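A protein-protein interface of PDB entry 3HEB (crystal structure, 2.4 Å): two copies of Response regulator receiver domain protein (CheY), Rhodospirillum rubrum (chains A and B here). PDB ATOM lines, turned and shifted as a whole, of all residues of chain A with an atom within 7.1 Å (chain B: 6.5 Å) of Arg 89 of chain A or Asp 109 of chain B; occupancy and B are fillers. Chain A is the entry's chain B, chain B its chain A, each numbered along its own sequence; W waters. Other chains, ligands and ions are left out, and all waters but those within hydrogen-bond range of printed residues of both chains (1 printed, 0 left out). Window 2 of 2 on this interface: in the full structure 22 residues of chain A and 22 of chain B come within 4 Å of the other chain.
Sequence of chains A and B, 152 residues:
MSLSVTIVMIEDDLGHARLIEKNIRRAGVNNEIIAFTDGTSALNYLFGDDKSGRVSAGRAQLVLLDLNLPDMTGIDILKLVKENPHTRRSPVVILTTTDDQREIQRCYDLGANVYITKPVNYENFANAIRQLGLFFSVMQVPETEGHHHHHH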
ATOM      1  N   ARG A  59      28.891 -16.673   2.791  1.00  0.00           N
ATOM      2  CA  ARG A  59      28.477 -18.026   2.454  1.00  0.00           C
ATOM      3  C   ARG A  59      28.764 -18.408   1.003  1.00  0.00           C
ATOM      4  O   ARG A  59      28.614 -17.599   0.089  1.00  0.00           O
ATOM      5  CB  ARG A  59      26.979 -18.191   2.684  1.00  0.00           C
ATOM      6  CG  ARG A  59      26.529 -18.349   4.124  1.00  0.00           C
ATOM      7  CD  ARG A  59      25.010 -18.434   4.102  1.00  0.00           C
ATOM      8  NE  ARG A  59      24.430 -18.886   5.355  1.00  0.00           N
ATOM      9  CZ  ARG A  59      23.132 -18.823   5.630  1.00  0.00           C
ATOM     10  NH1 ARG A  59      22.280 -18.320   4.741  1.00  0.00           N
ATOM     11  NH2 ARG A  59      22.683 -19.273   6.792  1.00  0.00           N
ATOM     12  N   GLN A  61      27.244 -20.725  -1.470  1.00  0.00           N
ATOM     13  CA  GLN A  61      26.070 -21.553  -1.695  1.00  0.00           C
ATOM     14  C   GLN A  61      25.534 -21.397  -3.103  1.00  0.00           C
ATOM     15  O   GLN A  61      25.750 -20.388  -3.757  1.00  0.00           O
ATOM     16  CB  GLN A  61      24.975 -21.155  -0.711  1.00  0.00           C
ATOM     17  CG  GLN A  61      24.658 -19.649  -0.771  1.00  0.00           C
ATOM     18  CD  GLN A  61      23.829 -19.130   0.403  1.00  0.00           C
ATOM     19  OE1 GLN A  61      23.583 -19.842   1.381  1.00  0.00           O
ATOM     20  NE2 GLN A  61      23.413 -17.871   0.312  1.00  0.00           N
ATOM     21  N   VAL A  81      17.298 -12.133  -4.051  1.00  0.00           N
ATOM     22  CA  VAL A  81      18.647 -12.681  -3.992  1.00  0.00           C
ATOM     23  C   VAL A  81      19.671 -11.895  -4.810  1.00  0.00           C
ATOM     24  O   VAL A  81      20.755 -11.582  -4.310  1.00  0.00           O
ATOM     25  CB  VAL A  81      18.674 -14.162  -4.466  1.00  0.00           C
ATOM     26  CG1 VAL A  81      20.108 -14.643  -4.603  1.00  0.00           C
ATOM     27  CG2 VAL A  81      17.935 -15.038  -3.490  1.00  0.00           C
ATOM     28  N   LYS A  82      19.342 -11.581  -6.062  1.00  0.00           N
ATOM     29  CA  LYS A  82      20.276 -10.851  -6.918  1.00  0.00           C
ATOM     30  C   LYS A  82      20.361  -9.357  -6.616  1.00  0.00           C
ATOM     31  O   LYS A  82      21.145  -8.638  -7.224  1.00  0.00           O
ATOM     32  CB  LYS A  82      19.925 -11.046  -8.393  1.00  0.00           C
ATOM     33  CG  LYS A  82      19.575 -12.476  -8.778  1.00  0.00           C
ATOM     34  CD  LYS A  82      20.601 -13.501  -8.300  1.00  0.00           C
ATOM     35  CE  LYS A  82      21.936 -13.382  -8.996  1.00  0.00           C
ATOM     36  NZ  LYS A  82      22.806 -14.546  -8.645  1.00  0.00           N
ATOM     37  N   ASN A  84      20.292  -8.178  -3.097  1.00  0.00           N
ATOM     38  CA  ASN A  84      21.032  -8.086  -1.843  1.00  0.00           C
ATOM     39  C   ASN A  84      22.528  -8.341  -2.038  1.00  0.00           C
ATOM     40  O   ASN A  84      22.924  -9.309  -2.681  1.00  0.00           O
ATOM     41  CB  ASN A  84      20.471  -9.088  -0.834  1.00  0.00           C
ATOM     42  CG  ASN A  84      20.880  -8.780   0.590  1.00  0.00           C
ATOM     43  OD1 ASN A  84      20.190  -8.049   1.300  1.00  0.00           O
ATOM     44  ND2 ASN A  84      22.013  -9.326   1.015  1.00  0.00           N
ATOM     45  N   PRO A  85      23.379  -7.472  -1.471  1.00  0.00           N
ATOM     46  CA  PRO A  85      24.836  -7.602  -1.581  1.00  0.00           C
ATOM     47  C   PRO A  85      25.435  -8.807  -0.853  1.00  0.00           C
ATOM     48  O   PRO A  85      26.593  -9.161  -1.094  1.00  0.00           O
ATOM     49  CB  PRO A  85      25.345  -6.277  -1.019  1.00  0.00           C
ATOM     50  CG  PRO A  85      24.301  -5.934   0.012  1.00  0.00           C
ATOM     51  CD  PRO A  85      23.014  -6.257  -0.723  1.00  0.00           C
ATOM     52  N   HIS A  86      24.660  -9.437   0.024  1.00  0.00           N
ATOM     53  CA  HIS A  86      25.153 -10.602   0.763  1.00  0.00           C
ATOM     54  C   HIS A  86      24.648 -11.941   0.207  1.00  0.00           C
ATOM     55  O   HIS A  86      24.940 -13.001   0.773  1.00  0.00           O
ATOM     56  CB  HIS A  86      24.783 -10.493   2.247  1.00  0.00           C
ATOM     57  CG  HIS A  86      25.283  -9.246   2.903  1.00  0.00           C
ATOM     58  ND1 HIS A  86      26.611  -8.872   2.879  1.00  0.00           N
ATOM     59  CD2 HIS A  86      24.629  -8.271   3.583  1.00  0.00           C
ATOM     60  CE1 HIS A  86      26.753  -7.721   3.514  1.00  0.00           C
ATOM     61  NE2 HIS A  86      25.566  -7.337   3.949  1.00  0.00           N
ATOM     62  N   THR A  87      23.897 -11.889  -0.892  1.00  0.00           N
ATOM     63  CA  THR A  87      23.371 -13.098  -1.517  1.00  0.00           C
ATOM     64  C   THR A  87      23.501 -13.079  -3.040  1.00  0.00           C
ATOM     65  O   THR A  87      23.597 -14.135  -3.676  1.00  0.00           O
ATOM     66  CB  THR A  87      21.875 -13.302  -1.199  1.00  0.00           C
ATOM     67  OG1 THR A  87      21.138 -12.160  -1.646  1.00  0.00           O
ATOM     68  CG2 THR A  87      21.647 -13.498   0.288  1.00  0.00           C
ATOM     69  N   ARG A  88      23.526 -11.884  -3.624  1.00  0.00           N
ATOM     70  CA  ARG A  88      23.576 -11.757  -5.077  1.00  0.00           C
ATOM     71  C   ARG A  88      24.645 -12.554  -5.813  1.00  0.00           C
ATOM     72  O   ARG A  88      24.398 -13.030  -6.920  1.00  0.00           O
ATOM     73  CB  ARG A  88      23.660 -10.284  -5.486  1.00  0.00           C
ATOM     74  CG  ARG A  88      24.901  -9.561  -5.031  1.00  0.00           C
ATOM     75  CD  ARG A  88      24.794  -8.082  -5.346  1.00  0.00           C
ATOM     76  NE  ARG A  88      26.006  -7.371  -4.948  1.00  0.00           N
ATOM     77  CZ  ARG A  88      26.096  -6.051  -4.809  1.00  0.00           C
ATOM     78  NH1 ARG A  88      25.038  -5.275  -5.041  1.00  0.00           N
ATOM     79  NH2 ARG A  88      27.244  -5.510  -4.418  1.00  0.00           N
ATOM     80  N   ARG A  89      25.811 -12.718  -5.196  1.00  0.00           N
ATOM     81  CA  ARG A  89      26.913 -13.449  -5.821  1.00  0.00           C
ATOM     82  C   ARG A  89      26.669 -14.962  -5.838  1.00  0.00           C
ATOM     83  O   ARG A  89      27.384 -15.711  -6.503  1.00  0.00           O
ATOM     84  CB  ARG A  89      28.222 -13.133  -5.082  1.00  0.00           C
ATOM     85  CG  ARG A  89      29.491 -13.606  -5.769  1.00  0.00           C
ATOM     86  CD  ARG A  89      30.716 -13.276  -4.920  1.00  0.00           C
ATOM     87  NE  ARG A  89      30.991 -11.842  -4.867  1.00  0.00           N
ATOM     88  CZ  ARG A  89      31.800 -11.274  -3.977  1.00  0.00           C
ATOM     89  NH1 ARG A  89      32.399 -12.021  -3.066  1.00  0.00           N
ATOM     90  NH2 ARG A  89      32.030  -9.970  -4.009  1.00  0.00           N
ATOM     91  N   SER A  90      25.659 -15.414  -5.104  1.00  0.00           N
ATOM     92  CA  SER A  90      25.359 -16.838  -5.074  1.00  0.00           C
ATOM     93  C   SER A  90      24.765 -17.249  -6.411  1.00  0.00           C
ATOM     94  O   SER A  90      23.835 -16.614  -6.902  1.00  0.00           O
ATOM     95  CB  SER A  90      24.371 -17.150  -3.957  1.00  0.00           C
ATOM     96  OG  SER A  90      24.956 -16.921  -2.694  1.00  0.00           O
ATOM     97  N   PRO A  91      25.312 -18.301  -7.034  1.00  0.00           N
ATOM     98  CA  PRO A  91      24.762 -18.732  -8.326  1.00  0.00           C
ATOM     99  C   PRO A  91      23.369 -19.319  -8.154  1.00  0.00           C
ATOM    100  O   PRO A  91      23.166 -20.220  -7.343  1.00  0.00           O
ATOM    101  CB  PRO A  91      25.777 -19.766  -8.813  1.00  0.00           C
ATOM    102  CG  PRO A  91      26.316 -20.326  -7.536  1.00  0.00           C
ATOM    103  CD  PRO A  91      26.509 -19.083  -6.690  1.00  0.00           C
ATOM    104  N   VAL A  92      22.415 -18.787  -8.909  1.00  0.00           N
ATOM    105  CA  VAL A  92      21.046 -19.262  -8.850  1.00  0.00           C
ATOM    106  C   VAL A  92      20.714 -20.032 -10.112  1.00  0.00           C
ATOM    107  O   VAL A  92      20.859 -19.513 -11.223  1.00  0.00           O
ATOM    108  CB  VAL A  92      20.039 -18.092  -8.720  1.00  0.00           C
ATOM    109  CG1 VAL A  92      18.604 -18.629  -8.767  1.00  0.00           C
ATOM    110  CG2 VAL A  92      20.274 -17.341  -7.415  1.00  0.00           C
ATOM    111  N   ASN A 113      21.692 -17.397 -12.988  1.00  0.00           N
ATOM    112  CA  ASN A 113      22.939 -17.858 -13.588  1.00  0.00           C
ATOM    113  C   ASN A 113      22.656 -18.890 -14.668  1.00  0.00           C
ATOM    114  O   ASN A 113      23.294 -18.887 -15.725  1.00  0.00           O
ATOM    115  CB  ASN A 113      23.848 -18.504 -12.530  1.00  0.00           C
ATOM    116  CG  ASN A 113      24.401 -17.504 -11.537  1.00  0.00           C
ATOM    117  OD1 ASN A 113      25.562 -17.097 -11.631  1.00  0.00           O
ATOM    118  ND2 ASN A 113      23.565 -17.096 -10.574  1.00  0.00           N
ATOM    119  N   VAL A 141      31.954 -22.100  -6.934  1.00  0.00           N
ATOM    120  CA  VAL A 141      30.838 -21.447  -6.260  1.00  0.00           C
ATOM    121  C   VAL A 141      31.494 -20.457  -5.307  1.00  0.00           C
ATOM    122  O   VAL A 141      32.198 -20.853  -4.375  1.00  0.00           O
ATOM    123  CB  VAL A 141      29.979 -22.456  -5.471  1.00  0.00           C
ATOM    124  CG1 VAL A 141      28.908 -21.720  -4.691  1.00  0.00           C
ATOM    125  CG2 VAL A 141      29.327 -23.438  -6.432  1.00  0.00           C
ATOM    126  N   PRO A 142      31.271 -19.150  -5.524  1.00  0.00           N
ATOM    127  CA  PRO A 142      31.870 -18.120  -4.675  1.00  0.00           C
ATOM    128  C   PRO A 142      31.112 -17.783  -3.402  1.00  0.00           C
ATOM    129  O   PRO A 142      29.923 -18.062  -3.272  1.00  0.00           O
ATOM    130  CB  PRO A 142      31.930 -16.929  -5.610  1.00  0.00           C
ATOM    131  CG  PRO A 142      30.596 -17.029  -6.290  1.00  0.00           C
ATOM    132  CD  PRO A 142      30.443 -18.531  -6.577  1.00  0.00           C
ATOM    133  N   GLU A 143      31.832 -17.182  -2.459  1.00  0.00           N
ATOM    134  CA  GLU A 143      31.243 -16.739  -1.205  1.00  0.00           C
ATOM    135  C   GLU A 143      30.731 -15.337  -1.508  1.00  0.00           C
ATOM    136  O   GLU A 143      31.319 -14.601  -2.310  1.00  0.00           O
ATOM    137  CB  GLU A 143      32.293 -16.634  -0.103  1.00  0.00           C
ATOM    138  CG  GLU A 143      33.161 -17.853   0.087  1.00  0.00           C
ATOM    139  CD  GLU A 143      34.267 -17.602   1.095  1.00  0.00           C
ATOM    140  OE1 GLU A 143      34.870 -16.507   1.050  1.00  0.00           O
ATOM    141  OE2 GLU A 143      34.541 -18.492   1.925  1.00  0.00           O
ATOM    142  N   THR A 144      29.643 -14.959  -0.862  1.00  0.00           N
ATOM    143  CA  THR A 144      29.086 -13.643  -1.074  1.00  0.00           C
ATOM    144  C   THR A 144      29.893 -12.637  -0.257  1.00  0.00           C
ATOM    145  O   THR A 144      30.839 -13.013   0.440  1.00  0.00           O
ATOM    146  CB  THR A 144      27.643 -13.626  -0.621  1.00  0.00           C
ATOM    147  OG1 THR A 144      27.596 -14.032   0.748  1.00  0.00           O
ATOM    148  CG2 THR A 144      26.810 -14.598  -1.468  1.00  0.00           C
ATOM    149  N   GLU A 145      29.520 -11.366  -0.340  1.00  0.00           N
ATOM    150  CA  GLU A 145      30.208 -10.322   0.403  1.00  0.00           C
ATOM    151  C   GLU A 145      29.930 -10.466   1.894  1.00  0.00           C
ATOM    152  O   GLU A 145      28.936 -11.070   2.279  1.00  0.00           O
ATOM    153  CB  GLU A 145      29.747  -8.950  -0.086  1.00  0.00           C
ATOM    154  CG  GLU A 145      29.824  -8.777  -1.602  1.00  0.00           C
ATOM    155  CD  GLU A 145      29.400  -7.386  -2.058  1.00  0.00           C
ATOM    156  OE1 GLU A 145      29.175  -7.200  -3.275  1.00  0.00           O
ATOM    157  OE2 GLU A 145      29.299  -6.479  -1.199  1.00  0.00           O
ATOM    158  N   GLY A 146      30.810  -9.912   2.728  1.00  0.00           N
ATOM    159  CA  GLY A 146      30.637  -9.987   4.173  1.00  0.00           C
ATOM    160  C   GLY A 146      30.067  -8.716   4.785  1.00  0.00           C
ATOM    161  O   GLY A 146      29.430  -8.747   5.848  1.00  0.00           O
ATOM    162  N   GLN B 101      39.947 -16.568  -5.105  1.00  0.00           N
ATOM    163  CA  GLN B 101      38.669 -15.941  -4.772  1.00  0.00           C
ATOM    164  C   GLN B 101      38.406 -14.603  -5.458  1.00  0.00           C
ATOM    165  O   GLN B 101      37.380 -14.430  -6.117  1.00  0.00           O
ATOM    166  CB  GLN B 101      38.561 -15.709  -3.259  1.00  0.00           C
ATOM    167  CG  GLN B 101      39.328 -16.683  -2.382  1.00  0.00           C
ATOM    168  CD  GLN B 101      39.529 -16.147  -0.957  1.00  0.00           C
ATOM    169  OE1 GLN B 101      40.050 -15.038  -0.754  1.00  0.00           O
ATOM    170  NE2 GLN B 101      39.120 -16.942   0.036  1.00  0.00           N
ATOM    171  N   ILE B 104      37.431 -14.871  -9.130  1.00  0.00           N
ATOM    172  CA  ILE B 104      36.173 -15.564  -9.266  1.00  0.00           C
ATOM    173  C   ILE B 104      35.045 -14.636  -8.846  1.00  0.00           C
ATOM    174  O   ILE B 104      34.105 -14.413  -9.612  1.00  0.00           O
ATOM    175  CB  ILE B 104      36.178 -16.850  -8.408  1.00  0.00           C
ATOM    176  CG1 ILE B 104      37.249 -17.814  -8.944  1.00  0.00           C
ATOM    177  CG2 ILE B 104      34.817 -17.495  -8.427  1.00  0.00           C
ATOM    178  CD1 ILE B 104      37.405 -19.095  -8.142  1.00  0.00           C
ATOM    179  N   GLN B 105      35.155 -14.076  -7.645  1.00  0.00           N
ATOM    180  CA  GLN B 105      34.133 -13.171  -7.131  1.00  0.00           C
ATOM    181  C   GLN B 105      33.920 -11.958  -8.042  1.00  0.00           C
ATOM    182  O   GLN B 105      32.787 -11.494  -8.214  1.00  0.00           O
ATOM    183  CB  GLN B 105      34.508 -12.701  -5.722  1.00  0.00           C
ATOM    184  CG  GLN B 105      34.904 -13.840  -4.782  1.00  0.00           C
ATOM    185  CD  GLN B 105      35.273 -13.362  -3.382  1.00  0.00           C
ATOM    186  OE1 GLN B 105      35.967 -12.346  -3.206  1.00  0.00           O
ATOM    187  NE2 GLN B 105      34.824 -14.108  -2.376  1.00  0.00           N
ATOM    188  N   ARG B 106      35.002 -11.452  -8.628  1.00  0.00           N
ATOM    189  CA  ARG B 106      34.913 -10.292  -9.506  1.00  0.00           C
ATOM    190  C   ARG B 106      34.126 -10.620 -10.787  1.00  0.00           C
ATOM    191  O   ARG B 106      33.296  -9.822 -11.241  1.00  0.00           O
ATOM    192  CB  ARG B 106      36.320  -9.793  -9.858  1.00  0.00           C
ATOM    193  CG  ARG B 106      36.372  -8.334 -10.296  1.00  0.00           C
ATOM    194  CD  ARG B 106      37.805  -7.890 -10.616  1.00  0.00           C
ATOM    195  NE  ARG B 106      37.935  -6.429 -10.685  1.00  0.00           N
ATOM    196  CZ  ARG B 106      38.260  -5.649  -9.653  1.00  0.00           C
ATOM    197  NH1 ARG B 106      38.500  -6.178  -8.457  1.00  0.00           N
ATOM    198  NH2 ARG B 106      38.344  -4.333  -9.813  1.00  0.00           N
ATOM    199  N   CYS B 107      34.389 -11.792 -11.362  1.00  0.00           N
ATOM    200  CA  CYS B 107      33.695 -12.229 -12.571  1.00  0.00           C
ATOM    201  C   CYS B 107      32.194 -12.333 -12.295  1.00  0.00           C
ATOM    202  O   CYS B 107      31.368 -11.849 -13.073  1.00  0.00           O
ATOM    203  CB  CYS B 107      34.242 -13.580 -13.050  1.00  0.00           C
ATOM    204  SG  CYS B 107      35.941 -13.499 -13.717  1.00  0.00           S
ATOM    205  N   TYR B 108      31.836 -12.963 -11.182  1.00  0.00           N
ATOM    206  CA  TYR B 108      30.428 -13.061 -10.855  1.00  0.00           C
ATOM    207  C   TYR B 108      29.849 -11.654 -10.639  1.00  0.00           C
ATOM    208  O   TYR B 108      28.759 -11.351 -11.117  1.00  0.00           O
ATOM    209  CB  TYR B 108      30.229 -13.941  -9.619  1.00  0.00           C
ATOM    210  CG  TYR B 108      30.361 -15.421  -9.910  1.00  0.00           C
ATOM    211  CD1 TYR B 108      31.484 -16.147  -9.496  1.00  0.00           C
ATOM    212  CD2 TYR B 108      29.354 -16.104 -10.589  1.00  0.00           C
ATOM    213  CE1 TYR B 108      31.590 -17.525  -9.748  1.00  0.00           C
ATOM    214  CE2 TYR B 108      29.451 -17.473 -10.853  1.00  0.00           C
ATOM    215  CZ  TYR B 108      30.567 -18.178 -10.427  1.00  0.00           C
ATOM    216  OH  TYR B 108      30.651 -19.531 -10.672  1.00  0.00           O
ATOM    217  N   ASP B 109      30.579 -10.792  -9.936  1.00  0.00           N
ATOM    218  CA  ASP B 109      30.089  -9.440  -9.717  1.00  0.00           C
ATOM    219  C   ASP B 109      29.917  -8.764 -11.062  1.00  0.00           C
ATOM    220  O   ASP B 109      28.963  -8.021 -11.257  1.00  0.00           O
ATOM    221  CB  ASP B 109      31.048  -8.625  -8.845  1.00  0.00           C
ATOM    222  CG  ASP B 109      31.084  -9.109  -7.401  1.00  0.00           C
ATOM    223  OD1 ASP B 109      30.146  -9.832  -6.973  1.00  0.00           O
ATOM    224  OD2 ASP B 109      32.046  -8.753  -6.691  1.00  0.00           O
ATOM    225  N   LEU B 110      30.836  -9.031 -11.991  1.00  0.00           N
ATOM    226  CA  LEU B 110      30.756  -8.457 -13.334  1.00  0.00           C
ATOM    227  C   LEU B 110      29.650  -9.087 -14.175  1.00  0.00           C
ATOM    228  O   LEU B 110      29.379  -8.626 -15.280  1.00  0.00           O
ATOM    229  CB  LEU B 110      32.084  -8.609 -14.084  1.00  0.00           C
ATOM    230  CG  LEU B 110      33.115  -7.473 -14.118  1.00  0.00           C
ATOM    231  CD1 LEU B 110      32.561  -6.205 -13.455  1.00  0.00           C
ATOM    232  CD2 LEU B 110      34.399  -7.943 -13.445  1.00  0.00           C
ATOM    233  N   GLY B 111      29.042 -10.160 -13.664  1.00  0.00           N
ATOM    234  CA  GLY B 111      27.949 -10.810 -14.379  1.00  0.00           C
ATOM    235  C   GLY B 111      28.143 -12.178 -15.015  1.00  0.00           C
ATOM    236  O   GLY B 111      27.253 -12.653 -15.723  1.00  0.00           O
ATOM    237  N   ALA B 112      29.278 -12.822 -14.785  1.00  0.00           N
ATOM    238  CA  ALA B 112      29.507 -14.142 -15.368  1.00  0.00           C
ATOM    239  C   ALA B 112      28.465 -15.114 -14.832  1.00  0.00           C
ATOM    240  O   ALA B 112      28.153 -15.104 -13.640  1.00  0.00           O
ATOM    241  CB  ALA B 112      30.898 -14.636 -15.022  1.00  0.00           C
HETATM  242  O   HOH W   1      28.416  -9.087  -4.769  1.00  0.00           O
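The guanidinium group (NH2) of Arg 89 of chain A is in salt-bridge range of the side-chain carboxylate (OD2) of Asp 109 of chain B, at 2.9 Å.
NE2 of Gln 105 of chain B lies close to NH1 of Arg 89 of chain A (3.3 Å).
The guanidinium group (NH1) of Arg 89 of chain A is in hydrogen-bond range of the backbone carbonyl oxygen (O) of Glu 143 of chain A.
The backbone NH (N) of Ala 112 of chain B sits at hydrogen-bond distance from the backbone carbonyl oxygen (O) of Cys 107 of chain B (2.9 Å).
The side-chain amide nitrogen (ND2) of Asn 113 of chain A sits close to the backbone NH (N) of Val 92 of chain A, 2.6 Å away.
The side-chain amino group (NZ) of Lys 82 of chain A sits close to the side-chain amide nitrogen (ND2) of Asn 113 of chain A, 3.3 Å away.
CG of Arg 89 of chain A touches CB of Tyr 108 of chain B, 3.9 Å away.
Tyr 108 of chain B touches Asn 113 of chain A (CE2 to OD1, 3.98 Å).
Asn 113 of chain A touches Ala 112 of chain B (OD1 to O, 3.8 Å).
Tyr 108 of chain B touches Pro 142 of chain A (CD1 to CG, 3.4 Å).
Glu 143 of chain A touches Gln 105 of chain B.
Arg 89 of chain A touches three residues of chain B.
Asp 109 of chain B touches just one residue of chain A: Arg 89 (2.9 Å).
Printed residues of chain B within 4 Å of Glu 143 of chain A: Gln 105.
Of the printed residues of chain B, Pro 142 of chain A touches Tyr 108.
Printed residues of chain A within 4 Å of Gln 105 of chain B: Arg 89 (3.2 Å) and Glu 143 (3.5 Å).
Printed residues of chain A within 4 Å of Ala 112 of chain B: Asn 113.
Thr 144 of chain A touches none of the printed residues of chain B.
The nearest residue of chain A that does not touch Asp 109 of chain B is Glu 145 of chain A (4.6 Å).
Of the 10 printed residues of chain B, 4 touch a printed residue of chain A.
Hydrophobic or aromatic side chains of chain A within 4 Å of the printed part of chain B: Pro 142.
Among the printed residues, 7 pairs touch across the chains.
Among the printed residues, Asp or Glu carboxylates within 4 Å of a Lys or Arg side-chain nitrogen of the other chain: Arg 89 of chain A with Asp 109 of chain B.
No position is printed for both chains.
Of the 7 pairs that touch across the chains among the printed residues, none has its exchanged pair printed and touching as well.
Water W1 lies within hydrogen-bond range of OE1 of Glu 145 of chain A (2.5 Å), OD1 of Asp 109 of chain B (2.9 Å) and NE of Arg 88 of chain A (3.0 Å).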
